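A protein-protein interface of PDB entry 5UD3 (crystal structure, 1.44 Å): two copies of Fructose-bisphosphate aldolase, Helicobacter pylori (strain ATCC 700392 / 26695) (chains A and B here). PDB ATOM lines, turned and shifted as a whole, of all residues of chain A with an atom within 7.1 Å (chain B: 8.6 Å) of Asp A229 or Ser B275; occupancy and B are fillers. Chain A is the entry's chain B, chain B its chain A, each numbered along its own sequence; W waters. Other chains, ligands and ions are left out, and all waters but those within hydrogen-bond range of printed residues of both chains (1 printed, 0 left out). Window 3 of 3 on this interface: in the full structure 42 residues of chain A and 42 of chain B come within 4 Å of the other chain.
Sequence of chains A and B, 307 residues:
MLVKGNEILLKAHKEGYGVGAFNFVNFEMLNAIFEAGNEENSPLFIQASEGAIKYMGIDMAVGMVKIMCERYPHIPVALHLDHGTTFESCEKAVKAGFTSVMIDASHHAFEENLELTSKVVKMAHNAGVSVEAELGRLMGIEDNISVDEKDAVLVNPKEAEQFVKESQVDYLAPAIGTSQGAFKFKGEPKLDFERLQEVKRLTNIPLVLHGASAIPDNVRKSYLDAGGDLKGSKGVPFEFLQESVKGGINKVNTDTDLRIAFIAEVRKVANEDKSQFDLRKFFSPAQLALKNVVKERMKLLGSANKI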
ATOM      1  N   PHE A 183      26.209   4.443 -24.797  1.00  0.00           N
ATOM      2  CA  PHE A 183      26.600   4.856 -26.144  1.00  0.00           C
ATOM      3  C   PHE A 183      27.799   5.793 -26.044  1.00  0.00           C
ATOM      4  O   PHE A 183      27.714   6.983 -26.376  1.00  0.00           O
ATOM      5  CB  PHE A 183      25.400   5.495 -26.853  1.00  0.00           C
ATOM      6  CG  PHE A 183      24.146   4.679 -26.734  1.00  0.00           C
ATOM      7  CD1 PHE A 183      23.910   3.618 -27.596  1.00  0.00           C
ATOM      8  CD2 PHE A 183      23.224   4.947 -25.738  1.00  0.00           C
ATOM      9  CE1 PHE A 183      22.763   2.850 -27.480  1.00  0.00           C
ATOM     10  CE2 PHE A 183      22.074   4.178 -25.608  1.00  0.00           C
ATOM     11  CZ  PHE A 183      21.844   3.133 -26.484  1.00  0.00           C
ATOM     12  N   TYR A 223      20.705  -9.412 -22.460  1.00  0.00           N
ATOM     13  CA  TYR A 223      19.721  -8.372 -22.742  1.00  0.00           C
ATOM     14  C   TYR A 223      19.074  -8.586 -24.106  1.00  0.00           C
ATOM     15  O   TYR A 223      17.848  -8.495 -24.249  1.00  0.00           O
ATOM     16  CB  TYR A 223      20.374  -6.988 -22.654  1.00  0.00           C
ATOM     17  CG  TYR A 223      19.370  -5.866 -22.606  1.00  0.00           C
ATOM     18  CD1 TYR A 223      18.685  -5.578 -21.439  1.00  0.00           C
ATOM     19  CD2 TYR A 223      19.101  -5.087 -23.732  1.00  0.00           C
ATOM     20  CE1 TYR A 223      17.752  -4.564 -21.391  1.00  0.00           C
ATOM     21  CE2 TYR A 223      18.163  -4.060 -23.687  1.00  0.00           C
ATOM     22  CZ  TYR A 223      17.485  -3.814 -22.508  1.00  0.00           C
ATOM     23  OH  TYR A 223      16.543  -2.818 -22.412  1.00  0.00           O
ATOM     24  N   LEU A 224      19.887  -8.878 -25.124  1.00  0.00           N
ATOM     25  CA  LEU A 224      19.347  -9.098 -26.460  1.00  0.00           C
ATOM     26  C   LEU A 224      18.526 -10.380 -26.530  1.00  0.00           C
ATOM     27  O   LEU A 224      17.490 -10.420 -27.205  1.00  0.00           O
ATOM     28  CB  LEU A 224      20.477  -9.131 -27.488  1.00  0.00           C
ATOM     29  CG  LEU A 224      20.768  -7.777 -28.136  1.00  0.00           C
ATOM     30  CD1 LEU A 224      21.125  -6.719 -27.098  1.00  0.00           C
ATOM     31  CD2 LEU A 224      21.868  -7.924 -29.183  1.00  0.00           C
ATOM     32  N   ALA A 226      16.670 -11.591 -24.381  1.00  0.00           N
ATOM     33  CA  ALA A 226      15.382 -11.300 -23.772  1.00  0.00           C
ATOM     34  C   ALA A 226      14.572 -10.272 -24.558  1.00  0.00           C
ATOM     35  O   ALA A 226      13.565  -9.771 -24.048  1.00  0.00           O
ATOM     36  CB  ALA A 226      15.579 -10.828 -22.329  1.00  0.00           C
ATOM     37  N   GLY A 227      14.990  -9.937 -25.780  1.00  0.00           N
ATOM     38  CA  GLY A 227      14.235  -9.025 -26.613  1.00  0.00           C
ATOM     39  C   GLY A 227      14.632  -7.569 -26.511  1.00  0.00           C
ATOM     40  O   GLY A 227      14.010  -6.726 -27.171  1.00  0.00           O
ATOM     41  N   GLY A 228      15.638  -7.242 -25.709  1.00  0.00           N
ATOM     42  CA  GLY A 228      16.053  -5.867 -25.580  1.00  0.00           C
ATOM     43  C   GLY A 228      16.852  -5.383 -26.772  1.00  0.00           C
ATOM     44  O   GLY A 228      17.382  -6.165 -27.560  1.00  0.00           O
ATOM     45  N   ASP A 229      16.932  -4.059 -26.885  1.00  0.00           N
ATOM     46  CA  ASP A 229      17.601  -3.376 -27.985  1.00  0.00           C
ATOM     47  C   ASP A 229      18.730  -2.540 -27.400  1.00  0.00           C
ATOM     48  O   ASP A 229      18.491  -1.681 -26.545  1.00  0.00           O
ATOM     49  CB  ASP A 229      16.604  -2.470 -28.716  1.00  0.00           C
ATOM     50  CG  ASP A 229      17.167  -1.871 -29.988  1.00  0.00           C
ATOM     51  OD1 ASP A 229      16.416  -1.136 -30.661  1.00  0.00           O
ATOM     52  OD2 ASP A 229      18.333  -2.150 -30.334  1.00  0.00           O
ATOM     53  N   LEU A 230      19.954  -2.793 -27.857  1.00  0.00           N
ATOM     54  CA  LEU A 230      21.120  -1.996 -27.491  1.00  0.00           C
ATOM     55  C   LEU A 230      21.825  -1.497 -28.743  1.00  0.00           C
ATOM     56  O   LEU A 230      23.056  -1.440 -28.804  1.00  0.00           O
ATOM     57  CB  LEU A 230      22.085  -2.794 -26.614  1.00  0.00           C
ATOM     58  CG  LEU A 230      21.600  -3.063 -25.191  1.00  0.00           C
ATOM     59  CD1 LEU A 230      22.398  -4.182 -24.544  1.00  0.00           C
ATOM     60  CD2 LEU A 230      21.696  -1.797 -24.366  1.00  0.00           C
ATOM     61  N   LYS A 231      21.053  -1.119 -29.760  1.00  0.00           N
ATOM     62  CA  LYS A 231      21.630  -0.755 -31.047  1.00  0.00           C
ATOM     63  C   LYS A 231      22.635   0.382 -30.891  1.00  0.00           C
ATOM     64  O   LYS A 231      22.301   1.455 -30.380  1.00  0.00           O
ATOM     65  CB  LYS A 231      20.519  -0.350 -32.014  1.00  0.00           C
ATOM     66  CG  LYS A 231      21.039   0.104 -33.369  1.00  0.00           C
ATOM     67  CD  LYS A 231      19.913   0.536 -34.287  1.00  0.00           C
ATOM     68  CE  LYS A 231      20.443   0.896 -35.656  1.00  0.00           C
ATOM     69  NZ  LYS A 231      20.511   2.363 -35.820  1.00  0.00           N
ATOM     70  N   GLY A 232      23.867   0.144 -31.345  1.00  0.00           N
ATOM     71  CA  GLY A 232      24.904   1.153 -31.325  1.00  0.00           C
ATOM     72  C   GLY A 232      25.652   1.294 -30.018  1.00  0.00           C
ATOM     73  O   GLY A 232      26.523   2.166 -29.915  1.00  0.00           O
ATOM     74  N   SER A 233      25.349   0.466 -29.025  1.00  0.00           N
ATOM     75  CA  SER A 233      25.970   0.607 -27.716  1.00  0.00           C
ATOM     76  C   SER A 233      27.455   0.260 -27.780  1.00  0.00           C
ATOM     77  O   SER A 233      27.891  -0.576 -28.579  1.00  0.00           O
ATOM     78  CB  SER A 233      25.283  -0.319 -26.714  1.00  0.00           C
ATOM     79  OG  SER A 233      25.565  -1.674 -27.026  1.00  0.00           O
ATOM     80  N   ARG A 267      13.092  -8.821 -18.090  1.00  0.00           N
ATOM     81  CA  ARG A 267      12.488  -9.061 -19.396  1.00  0.00           C
ATOM     82  C   ARG A 267      12.352 -10.549 -19.665  1.00  0.00           C
ATOM     83  O   ARG A 267      11.334 -11.001 -20.205  1.00  0.00           O
ATOM     84  CB  ARG A 267      13.343  -8.413 -20.491  1.00  0.00           C
ATOM     85  CG  ARG A 267      13.328  -6.895 -20.486  1.00  0.00           C
ATOM     86  CD  ARG A 267      14.259  -6.293 -21.552  1.00  0.00           C
ATOM     87  NE  ARG A 267      14.134  -4.843 -21.569  1.00  0.00           N
ATOM     88  CZ  ARG A 267      13.170  -4.175 -22.191  1.00  0.00           C
ATOM     89  NH1 ARG A 267      12.246  -4.818 -22.895  1.00  0.00           N
ATOM     90  NH2 ARG A 267      13.133  -2.853 -22.115  1.00  0.00           N
ATOM     91  N   VAL B 269       6.041  -1.513 -19.787  1.00  0.00           N
ATOM     92  CA  VAL B 269       7.256  -0.776 -20.143  1.00  0.00           C
ATOM     93  C   VAL B 269       8.188  -1.662 -20.956  1.00  0.00           C
ATOM     94  O   VAL B 269       8.783  -1.219 -21.952  1.00  0.00           O
ATOM     95  CB  VAL B 269       7.945  -0.212 -18.886  1.00  0.00           C
ATOM     96  CG1 VAL B 269       9.348   0.351 -19.219  1.00  0.00           C
ATOM     97  CG2 VAL B 269       7.065   0.844 -18.215  1.00  0.00           C
ATOM     98  N   ALA B 270       8.345  -2.918 -20.539  1.00  0.00           N
ATOM     99  CA  ALA B 270       9.218  -3.830 -21.269  1.00  0.00           C
ATOM    100  C   ALA B 270       8.747  -4.009 -22.704  1.00  0.00           C
ATOM    101  O   ALA B 270       9.564  -4.091 -23.630  1.00  0.00           O
ATOM    102  CB  ALA B 270       9.266  -5.180 -20.558  1.00  0.00           C
ATOM    103  N   ASN B 271       7.427  -4.059 -22.907  1.00  0.00           N
ATOM    104  CA  ASN B 271       6.869  -4.275 -24.239  1.00  0.00           C
ATOM    105  C   ASN B 271       7.077  -3.066 -25.135  1.00  0.00           C
ATOM    106  O   ASN B 271       7.365  -3.212 -26.330  1.00  0.00           O
ATOM    107  CB  ASN B 271       5.367  -4.525 -24.131  1.00  0.00           C
ATOM    108  CG  ASN B 271       5.029  -5.849 -23.508  1.00  0.00           C
ATOM    109  OD1 ASN B 271       5.872  -6.732 -23.373  1.00  0.00           O
ATOM    110  ND2 ASN B 271       3.768  -6.003 -23.134  1.00  0.00           N
ATOM    111  N   GLU B 272       6.908  -1.866 -24.590  1.00  0.00           N
ATOM    112  CA  GLU B 272       6.784  -0.671 -25.412  1.00  0.00           C
ATOM    113  C   GLU B 272       8.106   0.033 -25.681  1.00  0.00           C
ATOM    114  O   GLU B 272       8.152   0.885 -26.571  1.00  0.00           O
ATOM    115  CB  GLU B 272       5.805   0.310 -24.770  1.00  0.00           C
ATOM    116  CG  GLU B 272       4.411  -0.280 -24.648  1.00  0.00           C
ATOM    117  CD  GLU B 272       3.381   0.710 -24.160  1.00  0.00           C
ATOM    118  OE1 GLU B 272       3.747   1.687 -23.475  1.00  0.00           O
ATOM    119  OE2 GLU B 272       2.191   0.501 -24.466  1.00  0.00           O
ATOM    120  N   ASP B 273       9.170  -0.277 -24.941  1.00  0.00           N
ATOM    121  CA  ASP B 273      10.487   0.297 -25.227  1.00  0.00           C
ATOM    122  C   ASP B 273      11.537  -0.771 -24.946  1.00  0.00           C
ATOM    123  O   ASP B 273      11.936  -0.973 -23.797  1.00  0.00           O
ATOM    124  CB  ASP B 273      10.756   1.556 -24.418  1.00  0.00           C
ATOM    125  CG  ASP B 273      12.046   2.235 -24.832  1.00  0.00           C
ATOM    126  OD1 ASP B 273      12.757   1.663 -25.684  1.00  0.00           O
ATOM    127  OD2 ASP B 273      12.345   3.334 -24.320  1.00  0.00           O
ATOM    128  N   LYS B 274      11.989  -1.439 -26.004  1.00  0.00           N
ATOM    129  CA  LYS B 274      12.994  -2.480 -25.850  1.00  0.00           C
ATOM    130  C   LYS B 274      14.349  -1.919 -25.439  1.00  0.00           C
ATOM    131  O   LYS B 274      15.204  -2.684 -24.985  1.00  0.00           O
ATOM    132  CB  LYS B 274      13.105  -3.284 -27.148  1.00  0.00           C
ATOM    133  CG  LYS B 274      11.794  -3.928 -27.577  1.00  0.00           C
ATOM    134  CD  LYS B 274      11.237  -4.798 -26.462  1.00  0.00           C
ATOM    135  CE  LYS B 274      10.089  -5.676 -26.919  1.00  0.00           C
ATOM    136  NZ  LYS B 274       9.638  -6.534 -25.786  1.00  0.00           N
ATOM    137  N   SER B 275      14.560  -0.611 -25.571  1.00  0.00           N
ATOM    138  CA  SER B 275      15.818   0.004 -25.171  1.00  0.00           C
ATOM    139  C   SER B 275      15.818   0.475 -23.724  1.00  0.00           C
ATOM    140  O   SER B 275      16.835   0.996 -23.261  1.00  0.00           O
ATOM    141  CB  SER B 275      16.151   1.196 -26.084  1.00  0.00           C
ATOM    142  OG  SER B 275      15.422   2.347 -25.699  1.00  0.00           O
ATOM    143  N   GLN B 276      14.718   0.309 -22.993  1.00  0.00           N
ATOM    144  CA  GLN B 276      14.595   0.898 -21.664  1.00  0.00           C
ATOM    145  C   GLN B 276      15.186  -0.036 -20.613  1.00  0.00           C
ATOM    146  O   GLN B 276      14.729  -1.176 -20.455  1.00  0.00           O
ATOM    147  CB  GLN B 276      13.129   1.185 -21.337  1.00  0.00           C
ATOM    148  CG  GLN B 276      12.919   1.874 -19.993  1.00  0.00           C
ATOM    149  CD  GLN B 276      13.588   3.236 -19.927  1.00  0.00           C
ATOM    150  OE1 GLN B 276      14.654   3.390 -19.321  1.00  0.00           O
ATOM    151  NE2 GLN B 276      12.955   4.234 -20.526  1.00  0.00           N
ATOM    152  N   PHE B 277      16.167   0.464 -19.863  1.00  0.00           N
ATOM    153  CA  PHE B 277      16.716  -0.303 -18.750  1.00  0.00           C
ATOM    154  C   PHE B 277      16.910   0.513 -17.475  1.00  0.00           C
ATOM    155  O   PHE B 277      17.579   0.031 -16.554  1.00  0.00           O
ATOM    156  CB  PHE B 277      18.000  -1.048 -19.134  1.00  0.00           C
ATOM    157  CG  PHE B 277      19.037  -0.193 -19.822  1.00  0.00           C
ATOM    158  CD1 PHE B 277      19.858   0.651 -19.092  1.00  0.00           C
ATOM    159  CD2 PHE B 277      19.211  -0.269 -21.189  1.00  0.00           C
ATOM    160  CE1 PHE B 277      20.822   1.430 -19.726  1.00  0.00           C
ATOM    161  CE2 PHE B 277      20.159   0.503 -21.825  1.00  0.00           C
ATOM    162  CZ  PHE B 277      20.972   1.350 -21.093  1.00  0.00           C
ATOM    163  N   ASP B 278      16.340   1.711 -17.375  1.00  0.00           N
ATOM    164  CA  ASP B 278      16.340   2.458 -16.121  1.00  0.00           C
ATOM    165  C   ASP B 278      15.261   1.863 -15.223  1.00  0.00           C
ATOM    166  O   ASP B 278      14.069   1.943 -15.543  1.00  0.00           O
ATOM    167  CB  ASP B 278      16.046   3.928 -16.405  1.00  0.00           C
ATOM    168  CG  ASP B 278      16.116   4.815 -15.162  1.00  0.00           C
ATOM    169  OD1 ASP B 278      16.024   4.321 -14.019  1.00  0.00           O
ATOM    170  OD2 ASP B 278      16.258   6.043 -15.345  1.00  0.00           O
ATOM    171  N   PHE B 282      10.557   1.615 -15.112  1.00  0.00           N
ATOM    172  CA  PHE B 282       9.654   0.484 -14.921  1.00  0.00           C
ATOM    173  C   PHE B 282       8.839   0.637 -13.649  1.00  0.00           C
ATOM    174  O   PHE B 282       7.632   0.377 -13.644  1.00  0.00           O
ATOM    175  CB  PHE B 282      10.448  -0.814 -14.801  1.00  0.00           C
ATOM    176  CG  PHE B 282      11.072  -1.269 -16.083  1.00  0.00           C
ATOM    177  CD1 PHE B 282      12.295  -0.755 -16.506  1.00  0.00           C
ATOM    178  CD2 PHE B 282      10.447  -2.217 -16.864  1.00  0.00           C
ATOM    179  CE1 PHE B 282      12.870  -1.187 -17.691  1.00  0.00           C
ATOM    180  CE2 PHE B 282      11.012  -2.649 -18.035  1.00  0.00           C
ATOM    181  CZ  PHE B 282      12.229  -2.128 -18.458  1.00  0.00           C
HETATM  182  O   HOH W   1      11.890  -7.581 -23.794  1.00  0.00           O
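NH1 of Arg A267 sits at hydrogen-bond distance from O of Ala B270, at 2.9 Å. The backbone carbonyl oxygen of Asp B273 sits at hydrogen-bond distance from the guanidinium group of Arg A267 (2.8 Å). OH of Tyr A223 is in hydrogen-bond range of O of Lys B274. O of Lys B274 lies within hydrogen-bond range of N of Asp A229 (2.9 Å). The side-chain hydroxyl (OH) of Tyr A223 sits at hydrogen-bond distance from the backbone carbonyl oxygen (O) of Gln B276, 3.1 Å away. O of Gln B276 is in hydrogen-bond range of NH2 of Arg A267.
Printed residues of chain B within 4 Å of Tyr A223: Lys B274 (2.9 Å), Ser B275 (3.6 Å), Gln B276 (3.1 Å) and Phe B277 (3.9 Å). Of the printed residues of chain B, Gly A227 touches Lys B274 (3.5 Å). Asp A229 touches just these residues of chain B: Lys B274 and Ser B275. Of the printed residues of chain B, Arg A267 touches Ala B270 (2.9 Å), Asp B273 (2.8 Å), Lys B274 (3.5 Å), Gln B276 (2.8 Å) and Phe B282 (3.8 Å). Of the printed residues of chain A, Ala B270 touches Arg A267. The nearest residue of chain B that does not touch Asp A229 is Phe B277 (5.5 Å). The nearest printed residue of chain A that does not touch Lys B274 is Ala A226 (5.4 Å).
No position is printed for both chains.
NZ of Lys B274 is in hydrogen-bond range of O of Ala B270. The side-chain carboxylate (OD1) of Asp B273 sits at hydrogen-bond distance from the side-chain hydroxyl (OG) of Ser B275 (2.8 Å). N of Gly A228 is in hydrogen-bond range of O of Tyr A223 (2.9 Å). OH of Tyr A223 is in hydrogen-bond range of NE of Arg A267 (3.3 Å). OD2 of Asp A229 sits at hydrogen-bond distance from N of Lys A231 (3.0 Å). The side-chain hydroxyl (OG) of Ser A233 sits at hydrogen-bond distance from the backbone carbonyl oxygen (O) of Leu A230 (3.1 Å).
Water W1 lies within hydrogen-bond range of O of Ala A226, NH1 of Arg A267 and NZ of Lys B274.
Hydrophobic or aromatic side chains of chain A within 4 Å of the printed part of chain B: Tyr A223 and Leu A230. Among the printed residues, 14 pairs touch across the chains. Among the printed residues, no Asp or Glu carboxylate lies within 4 Å of a Lys or Arg side-chain nitrogen of the other chain.
Ser B275 touches Tyr A223 (C to OH, 3.6 Å). CD2 of Phe B277 touches OH of Tyr A223, 3.9 Å away. Lys B274 touches Gly A227. Lys B274 touches Gly A228. O of Asp A229 touches CA of Ser B275, 3.4 Å away. Leu A230 touches Phe B277 (CD2 to CE2, 3.8 Å). NH2 of Arg A267 touches O of Lys B274, at 3.5 Å. Arg A267 touches Phe B282 (NH2 to CZ, 3.8 Å).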
